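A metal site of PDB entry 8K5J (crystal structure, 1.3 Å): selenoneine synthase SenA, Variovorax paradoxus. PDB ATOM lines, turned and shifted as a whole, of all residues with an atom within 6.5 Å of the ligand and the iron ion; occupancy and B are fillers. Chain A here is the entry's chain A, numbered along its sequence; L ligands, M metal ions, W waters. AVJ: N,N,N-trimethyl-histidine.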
ATOM      1  N   TRP A  78     -12.323  -7.854  32.838  1.00  0.00           N
ATOM      2  CA  TRP A  78     -12.016  -7.387  31.494  1.00  0.00           C
ATOM      3  C   TRP A  78     -10.899  -8.249  30.896  1.00  0.00           C
ATOM      4  O   TRP A  78     -10.989  -8.675  29.734  1.00  0.00           O
ATOM      5  CB  TRP A  78     -11.662  -5.899  31.476  1.00  0.00           C
ATOM      6  CG  TRP A  78     -11.382  -5.394  30.106  1.00  0.00           C
ATOM      7  CD1 TRP A  78     -12.344  -4.959  29.225  1.00  0.00           C
ATOM      8  CD2 TRP A  78     -10.170  -5.484  29.339  1.00  0.00           C
ATOM      9  NE1 TRP A  78     -11.763  -4.692  28.016  1.00  0.00           N
ATOM     10  CE2 TRP A  78     -10.437  -5.002  28.046  1.00  0.00           C
ATOM     11  CE3 TRP A  78      -8.887  -5.888  29.629  1.00  0.00           C
ATOM     12  CZ2 TRP A  78      -9.446  -4.975  27.041  1.00  0.00           C
ATOM     13  CZ3 TRP A  78      -7.917  -5.869  28.674  1.00  0.00           C
ATOM     14  CH2 TRP A  78      -8.197  -5.412  27.380  1.00  0.00           C
ATOM     15  N   HIS A  82     -10.940 -10.348  27.454  1.00  0.00           N
ATOM     16  CA  HIS A  82      -9.955 -10.064  26.405  1.00  0.00           C
ATOM     17  C   HIS A  82      -9.249 -11.325  25.965  1.00  0.00           C
ATOM     18  O   HIS A  82      -8.963 -11.499  24.768  1.00  0.00           O
ATOM     19  CB  HIS A  82      -8.967  -9.001  26.907  1.00  0.00           C
ATOM     20  CG  HIS A  82      -7.825  -8.800  26.000  1.00  0.00           C
ATOM     21  ND1 HIS A  82      -7.894  -8.202  24.740  1.00  0.00           N
ATOM     22  CD2 HIS A  82      -6.533  -9.162  26.142  1.00  0.00           C
ATOM     23  CE1 HIS A  82      -6.656  -8.255  24.220  1.00  0.00           C
ATOM     24  NE2 HIS A  82      -5.821  -8.775  25.044  1.00  0.00           N
ATOM     25  N   PHE A  86      -9.517 -12.494  22.116  1.00  0.00           N
ATOM     26  CA  PHE A  86      -8.328 -12.601  21.266  1.00  0.00           C
ATOM     27  C   PHE A  86      -8.247 -13.976  20.637  1.00  0.00           C
ATOM     28  O   PHE A  86      -7.932 -14.116  19.425  1.00  0.00           O
ATOM     29  CB  PHE A  86      -7.095 -12.251  22.071  1.00  0.00           C
ATOM     30  CG  PHE A  86      -5.815 -12.184  21.271  1.00  0.00           C
ATOM     31  CD1 PHE A  86      -5.044 -13.299  21.050  1.00  0.00           C
ATOM     32  CD2 PHE A  86      -5.339 -10.984  20.786  1.00  0.00           C
ATOM     33  CE1 PHE A  86      -3.864 -13.259  20.327  1.00  0.00           C
ATOM     34  CE2 PHE A  86      -4.134 -10.933  20.076  1.00  0.00           C
ATOM     35  CZ  PHE A  86      -3.396 -12.064  19.887  1.00  0.00           C
ATOM     36  N   SER A 123      -8.297  -4.739  22.600  1.00  0.00           N
ATOM     37  CA  SER A 123      -7.352  -3.827  23.245  1.00  0.00           C
ATOM     38  C   SER A 123      -6.932  -2.727  22.318  1.00  0.00           C
ATOM     39  O   SER A 123      -6.393  -1.729  22.787  1.00  0.00           O
ATOM     40  CB  SER A 123      -6.243  -4.581  23.899  1.00  0.00           C
ATOM     41  OG  SER A 123      -5.600  -5.420  23.003  1.00  0.00           O
ATOM     42  N   HIS A 178      -0.199 -15.488  23.752  1.00  0.00           N
ATOM     43  CA  HIS A 178      -0.905 -14.283  24.218  1.00  0.00           C
ATOM     44  C   HIS A 178      -1.520 -14.525  25.592  1.00  0.00           C
ATOM     45  O   HIS A 178      -1.421 -13.674  26.486  1.00  0.00           O
ATOM     46  CB  HIS A 178      -1.985 -13.910  23.196  1.00  0.00           C
ATOM     47  CG  HIS A 178      -2.818 -12.752  23.620  1.00  0.00           C
ATOM     48  ND1 HIS A 178      -4.119 -12.895  24.101  1.00  0.00           N
ATOM     49  CD2 HIS A 178      -2.537 -11.437  23.682  1.00  0.00           C
ATOM     50  CE1 HIS A 178      -4.595 -11.652  24.412  1.00  0.00           C
ATOM     51  NE2 HIS A 178      -3.592 -10.734  24.203  1.00  0.00           N
ATOM     52  N   MET A 181       1.043 -14.422  28.311  1.00  0.00           N
ATOM     53  CA  MET A 181       1.438 -13.050  28.670  1.00  0.00           C
ATOM     54  C   MET A 181       0.418 -12.423  29.591  1.00  0.00           C
ATOM     55  O   MET A 181       0.808 -11.731  30.548  1.00  0.00           O
ATOM     56  CB  MET A 181       1.621 -12.205  27.409  1.00  0.00           C
ATOM     57  CG  MET A 181       2.721 -12.707  26.506  1.00  0.00           C
ATOM     58  SD  MET A 181       3.418 -11.818  25.239  1.00  0.00           S
ATOM     59  CE  MET A 181       2.956 -12.697  23.827  1.00  0.00           C
ATOM     60  N   HIS A 182      -0.848 -12.587  29.331  1.00  0.00           N
ATOM     61  CA  HIS A 182      -1.852 -12.006  30.237  1.00  0.00           C
ATOM     62  C   HIS A 182      -1.877 -12.727  31.577  1.00  0.00           C
ATOM     63  O   HIS A 182      -2.220 -12.069  32.583  1.00  0.00           O
ATOM     64  CB  HIS A 182      -3.238 -11.990  29.559  1.00  0.00           C
ATOM     65  CG  HIS A 182      -3.399 -10.868  28.593  1.00  0.00           C
ATOM     66  ND1 HIS A 182      -3.813  -9.595  28.970  1.00  0.00           N
ATOM     67  CD2 HIS A 182      -3.202 -10.764  27.260  1.00  0.00           C
ATOM     68  CE1 HIS A 182      -3.821  -8.802  27.916  1.00  0.00           C
ATOM     69  NE2 HIS A 182      -3.451  -9.476  26.823  1.00  0.00           N
ATOM     70  N   GLU A 184       0.860 -13.747  33.217  1.00  0.00           N
ATOM     71  CA  GLU A 184       1.923 -13.038  33.948  1.00  0.00           C
ATOM     72  C   GLU A 184       1.425 -11.647  34.341  1.00  0.00           C
ATOM     73  O   GLU A 184       1.758 -11.234  35.488  1.00  0.00           O
ATOM     74  CB  GLU A 184       3.165 -12.966  33.100  1.00  0.00           C
ATOM     75  CG  GLU A 184       4.280 -12.299  33.861  1.00  0.00           C
ATOM     76  CD  GLU A 184       5.498 -12.052  33.050  1.00  0.00           C
ATOM     77  OE1 GLU A 184       6.028 -10.910  33.081  1.00  0.00           O
ATOM     78  OE2 GLU A 184       5.978 -12.980  32.364  1.00  0.00           O
ATOM     79  N   ALA A 185       0.705 -10.938  33.505  1.00  0.00           N
ATOM     80  CA  ALA A 185       0.206  -9.616  33.890  1.00  0.00           C
ATOM     81  C   ALA A 185      -0.768  -9.740  35.085  1.00  0.00           C
ATOM     82  O   ALA A 185      -0.729  -8.866  35.961  1.00  0.00           O
ATOM     83  CB  ALA A 185      -0.479  -8.969  32.683  1.00  0.00           C
ATOM     84  N   TYR A 188       1.579  -9.775  38.113  1.00  0.00           N
ATOM     85  CA  TYR A 188       2.221  -8.576  38.584  1.00  0.00           C
ATOM     86  C   TYR A 188       1.155  -7.555  38.970  1.00  0.00           C
ATOM     87  O   TYR A 188       1.384  -6.769  39.925  1.00  0.00           O
ATOM     88  CB  TYR A 188       3.269  -7.982  37.642  1.00  0.00           C
ATOM     89  CG  TYR A 188       2.911  -7.522  36.263  1.00  0.00           C
ATOM     90  CD1 TYR A 188       2.232  -6.346  36.081  1.00  0.00           C
ATOM     91  CD2 TYR A 188       3.319  -8.222  35.139  1.00  0.00           C
ATOM     92  CE1 TYR A 188       1.923  -5.861  34.821  1.00  0.00           C
ATOM     93  CE2 TYR A 188       3.042  -7.736  33.863  1.00  0.00           C
ATOM     94  CZ  TYR A 188       2.380  -6.554  33.714  1.00  0.00           C
ATOM     95  OH  TYR A 188       2.089  -6.069  32.442  1.00  0.00           O
ATOM     96  N   TYR A 374      -1.064  -9.803  13.944  1.00  0.00           N
ATOM     97  CA  TYR A 374      -1.368  -8.943  15.104  1.00  0.00           C
ATOM     98  C   TYR A 374      -0.414  -7.766  15.052  1.00  0.00           C
ATOM     99  O   TYR A 374       0.646  -7.710  15.691  1.00  0.00           O
ATOM    100  CB  TYR A 374      -1.298  -9.731  16.411  1.00  0.00           C
ATOM    101  CG  TYR A 374      -1.566  -8.892  17.635  1.00  0.00           C
ATOM    102  CD1 TYR A 374      -2.344  -7.763  17.619  1.00  0.00           C
ATOM    103  CD2 TYR A 374      -1.072  -9.284  18.853  1.00  0.00           C
ATOM    104  CE1 TYR A 374      -2.572  -7.009  18.744  1.00  0.00           C
ATOM    105  CE2 TYR A 374      -1.281  -8.531  19.990  1.00  0.00           C
ATOM    106  CZ  TYR A 374      -2.043  -7.393  19.958  1.00  0.00           C
ATOM    107  OH  TYR A 374      -2.313  -6.673  21.078  1.00  0.00           O
ATOM    108  N   ASP A 376      -0.253  -4.730  15.971  1.00  0.00           N
ATOM    109  CA  ASP A 376       0.021  -3.865  17.101  1.00  0.00           C
ATOM    110  C   ASP A 376       0.849  -4.550  18.154  1.00  0.00           C
ATOM    111  O   ASP A 376       1.083  -3.936  19.202  1.00  0.00           O
ATOM    112  CB  ASP A 376      -1.249  -3.302  17.788  1.00  0.00           C
ATOM    113  CG  ASP A 376      -1.979  -2.174  17.154  1.00  0.00           C
ATOM    114  OD1 ASP A 376      -1.412  -1.681  16.108  1.00  0.00           O
ATOM    115  OD2 ASP A 376      -3.169  -1.770  17.725  1.00  0.00           O
ATOM    116  N   TYR A 377       1.293  -5.777  17.987  1.00  0.00           N
ATOM    117  CA  TYR A 377       2.089  -6.447  19.041  1.00  0.00           C
ATOM    118  C   TYR A 377       3.370  -5.696  19.356  1.00  0.00           C
ATOM    119  O   TYR A 377       3.699  -5.480  20.538  1.00  0.00           O
ATOM    120  CB  TYR A 377       2.354  -7.900  18.688  1.00  0.00           C
ATOM    121  CG  TYR A 377       3.143  -8.577  19.786  1.00  0.00           C
ATOM    122  CD1 TYR A 377       2.622  -8.804  21.059  1.00  0.00           C
ATOM    123  CD2 TYR A 377       4.429  -9.042  19.530  1.00  0.00           C
ATOM    124  CE1 TYR A 377       3.390  -9.357  22.065  1.00  0.00           C
ATOM    125  CE2 TYR A 377       5.196  -9.624  20.519  1.00  0.00           C
ATOM    126  CZ  TYR A 377       4.686  -9.748  21.797  1.00  0.00           C
ATOM    127  OH  TYR A 377       5.445 -10.296  22.820  1.00  0.00           O
ATOM    128  N   TRP A 381       5.354   0.245  19.693  1.00  0.00           N
ATOM    129  CA  TRP A 381       6.086   0.374  20.940  1.00  0.00           C
ATOM    130  C   TRP A 381       7.553   0.590  20.710  1.00  0.00           C
ATOM    131  O   TRP A 381       8.322   0.818  21.656  1.00  0.00           O
ATOM    132  CB  TRP A 381       5.829  -0.827  21.848  1.00  0.00           C
ATOM    133  CG  TRP A 381       4.408  -1.287  21.795  1.00  0.00           C
ATOM    134  CD1 TRP A 381       3.978  -2.451  21.230  1.00  0.00           C
ATOM    135  CD2 TRP A 381       3.210  -0.560  22.101  1.00  0.00           C
ATOM    136  NE1 TRP A 381       2.643  -2.522  21.218  1.00  0.00           N
ATOM    137  CE2 TRP A 381       2.145  -1.363  21.692  1.00  0.00           C
ATOM    138  CE3 TRP A 381       2.974   0.713  22.649  1.00  0.00           C
ATOM    139  CZ2 TRP A 381       0.829  -0.967  21.875  1.00  0.00           C
ATOM    140  CZ3 TRP A 381       1.630   1.134  22.772  1.00  0.00           C
ATOM    141  CH2 TRP A 381       0.597   0.273  22.421  1.00  0.00           C
ATOM    142  N   TYR A 404      13.354 -14.369  23.111  1.00  0.00           N
ATOM    143  CA  TYR A 404      12.185 -13.494  23.326  1.00  0.00           C
ATOM    144  C   TYR A 404      12.585 -12.145  23.766  1.00  0.00           C
ATOM    145  O   TYR A 404      13.446 -11.974  24.651  1.00  0.00           O
ATOM    146  CB  TYR A 404      11.287 -14.157  24.366  1.00  0.00           C
ATOM    147  CG  TYR A 404      10.028 -13.385  24.659  1.00  0.00           C
ATOM    148  CD1 TYR A 404       8.892 -13.604  23.929  1.00  0.00           C
ATOM    149  CD2 TYR A 404       9.964 -12.454  25.685  1.00  0.00           C
ATOM    150  CE1 TYR A 404       7.720 -12.886  24.169  1.00  0.00           C
ATOM    151  CE2 TYR A 404       8.819 -11.734  25.941  1.00  0.00           C
ATOM    152  CZ  TYR A 404       7.685 -11.977  25.206  1.00  0.00           C
ATOM    153  OH  TYR A 404       6.575 -11.213  25.497  1.00  0.00           O
ATOM    154  N   ARG A 405      11.968 -11.106  23.201  1.00  0.00           N
ATOM    155  CA  ARG A 405      12.249  -9.719  23.557  1.00  0.00           C
ATOM    156  C   ARG A 405      11.061  -9.176  24.312  1.00  0.00           C
ATOM    157  O   ARG A 405       9.998  -9.029  23.740  1.00  0.00           O
ATOM    158  CB  ARG A 405      12.479  -8.896  22.295  1.00  0.00           C
ATOM    159  CG  ARG A 405      13.553  -9.478  21.372  1.00  0.00           C
ATOM    160  CD  ARG A 405      13.704  -8.710  20.074  1.00  0.00           C
ATOM    161  NE  ARG A 405      14.391  -7.440  20.278  1.00  0.00           N
ATOM    162  CZ  ARG A 405      14.301  -6.407  19.463  1.00  0.00           C
ATOM    163  NH1 ARG A 405      13.460  -6.432  18.434  1.00  0.00           N
ATOM    164  NH2 ARG A 405      14.998  -5.294  19.712  1.00  0.00           N
ATOM    165  N   ASN A 406      11.203  -8.891  25.613  1.00  0.00           N
ATOM    166  CA  ASN A 406      10.189  -8.170  26.322  1.00  0.00           C
ATOM    167  C   ASN A 406      10.440  -6.690  26.181  1.00  0.00           C
ATOM    168  O   ASN A 406      11.560  -6.294  25.861  1.00  0.00           O
ATOM    169  CB  ASN A 406      10.067  -8.606  27.772  1.00  0.00           C
ATOM    170  CG  ASN A 406       8.664  -8.483  28.293  1.00  0.00           C
ATOM    171  OD1 ASN A 406       7.768  -7.904  27.681  1.00  0.00           O
ATOM    172  ND2 ASN A 406       8.412  -9.039  29.464  1.00  0.00           N
ATOM    173  N   PHE A 407       9.441  -5.853  26.450  1.00  0.00           N
ATOM    174  CA  PHE A 407       9.558  -4.427  26.169  1.00  0.00           C
ATOM    175  C   PHE A 407       8.565  -3.661  27.035  1.00  0.00           C
ATOM    176  O   PHE A 407       7.376  -3.860  26.916  1.00  0.00           O
ATOM    177  CB  PHE A 407       9.379  -4.133  24.653  1.00  0.00           C
ATOM    178  CG  PHE A 407       8.234  -4.829  23.976  1.00  0.00           C
ATOM    179  CD1 PHE A 407       8.378  -6.124  23.485  1.00  0.00           C
ATOM    180  CD2 PHE A 407       7.016  -4.199  23.717  1.00  0.00           C
ATOM    181  CE1 PHE A 407       7.366  -6.743  22.811  1.00  0.00           C
ATOM    182  CE2 PHE A 407       5.981  -4.854  23.049  1.00  0.00           C
ATOM    183  CZ  PHE A 407       6.196  -6.122  22.584  1.00  0.00           C
ATOM    184  N   PHE A 408       9.120  -2.774  27.854  1.00  0.00           N
ATOM    185  CA  PHE A 408       8.346  -1.887  28.754  1.00  0.00           C
ATOM    186  C   PHE A 408       9.069  -0.554  28.761  1.00  0.00           C
ATOM    187  O   PHE A 408      10.271  -0.480  28.583  1.00  0.00           O
ATOM    188  CB  PHE A 408       8.222  -2.485  30.158  1.00  0.00           C
ATOM    189  CG  PHE A 408       7.167  -3.569  30.257  1.00  0.00           C
ATOM    190  CD1 PHE A 408       5.832  -3.185  30.420  1.00  0.00           C
ATOM    191  CD2 PHE A 408       7.491  -4.892  30.197  1.00  0.00           C
ATOM    192  CE1 PHE A 408       4.835  -4.164  30.528  1.00  0.00           C
ATOM    193  CE2 PHE A 408       6.482  -5.840  30.278  1.00  0.00           C
ATOM    194  CZ  PHE A 408       5.173  -5.469  30.448  1.00  0.00           C
HETATM  195  CAA AVJ L   1       4.411  -8.100  27.797  1.00  0.00           C
HETATM  196  CAB AVJ L   1       5.047  -6.065  26.652  1.00  0.00           C
HETATM  197  CAC AVJ L   1       5.055  -8.155  25.459  1.00  0.00           C
HETATM  198  OAH AVJ L   1       1.455  -5.257  26.218  1.00  0.00           O
HETATM  199  OAL AVJ L   1       2.147  -6.120  28.072  1.00  0.00           O
HETATM  200  CAM AVJ L   1      -0.519  -8.814  25.692  1.00  0.00           C
HETATM  201  CAP AVJ L   1       2.011  -8.436  26.005  1.00  0.00           C
HETATM  202  NAR AVJ L   1       0.491  -7.654  24.142  1.00  0.00           N
HETATM  203  NAT AVJ L   1      -1.471  -8.513  24.719  1.00  0.00           N
HETATM  204  CAX AVJ L   1       2.094  -6.067  26.849  1.00  0.00           C
HETATM  205  CAY AVJ L   1       0.677  -8.312  25.345  1.00  0.00           C
HETATM  206  CAZ AVJ L   1      -0.821  -7.815  23.805  1.00  0.00           C
HETATM  207  CBC AVJ L   1       2.847  -7.137  26.054  1.00  0.00           C
HETATM  208  NBE AVJ L   1       4.305  -7.389  26.511  1.00  0.00           N
HETATM  209 FE    FE M   1      -3.626  -8.794  24.865  1.00  0.00          FE
HETATM  210  O   HOH W   1       3.015  -3.401  24.619  1.00  0.00           O
HETATM  211  O   HOH W   2      -3.862  -8.102  22.831  1.00  0.00           O
HETATM  212  O   HOH W   3      -1.342  -5.254  25.887  1.00  0.00           O
HETATM  213  O   HOH W   4       0.721  -4.154  29.226  1.00  0.00           O
HETATM  214  O   HOH W   5      -3.693  -6.772  25.451  1.00  0.00           O
HETATM  215  O   HOH W   6       2.960  -9.834  30.335  1.00  0.00           O
HETATM  216  O   HOH W   7       1.654  -7.527  30.218  1.00  0.00           O
HETATM  217  O   HOH W   8       5.694  -9.822  30.492  1.00  0.00           O
HETATM  218  O   HOH W   9       2.146  -5.754  22.818  1.00  0.00           O
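The iron ion is bound by a ring nitrogen (NE2) of His 178 (2.1 Å), a ring nitrogen (NE2) of His 182 (2.1 Å), water W5 (2.1 Å), water W2 (2.2 Å), a nitrogen (NAT) of the ligand (2.2 Å) and a ring nitrogen (NE2) of His 82 (2.2 Å).
The side-chain hydroxyl of Tyr 377 is in hydrogen-bond range of the side-chain hydroxyl of Tyr 404 (3.0 Å). SD of Met 181 sits at hydrogen-bond distance from OH of Tyr 404. OH of Tyr 377 sits at hydrogen-bond distance from SD of Met 181 (3.5 Å). O of Tyr 377 lies close to NE1 of Trp 381.
SD of Met 181 touches CAP of the ligand, at 3.7 Å. Tyr 374 touches the ligand. OH of Tyr 377 touches CAC of the ligand (3.4 Å). Tyr 404 touches the ligand. OD1 of Asn 406 touches CAA of the ligand, at 3.4 Å. Phe 407 touches the ligand. CZ of Phe 408 touches CAA of the ligand, 3.8 Å away. Hydrophobic or aromatic side chains within 4 Å of the ligand: His 178, Met 181, His 182, Tyr 374, Tyr 377, Phe 407 and Phe 408. Nine residues have an atom within 4 Å of the ligand: His 178, Met 181, His 182, Tyr 374, Tyr 377, Tyr 404, Asn 406, Phe 407 and Phe 408.
Within 4 Å of the iron ion: His 82, His 178 and His 182. The nearest printed residue that does not touch the iron ion is Ser 123 (4.3 Å).
Water W2 bridges the side-chain hydroxyl of Tyr 374 and the side-chain hydroxyl of Ser 123. Water W7 bridges an oxygen (OAL) of the ligand and the side-chain hydroxyl (OH) of Tyr 188. Water W9 bridges O of Tyr 377 (2.8 Å) and NAR of the ligand (2.8 Å). Water W8 lies within hydrogen-bond range of the side-chain carboxylate (OE1) of Glu 184 (2.8 Å) and the side-chain amide nitrogen (ND2) of Asn 406 (3.0 Å).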
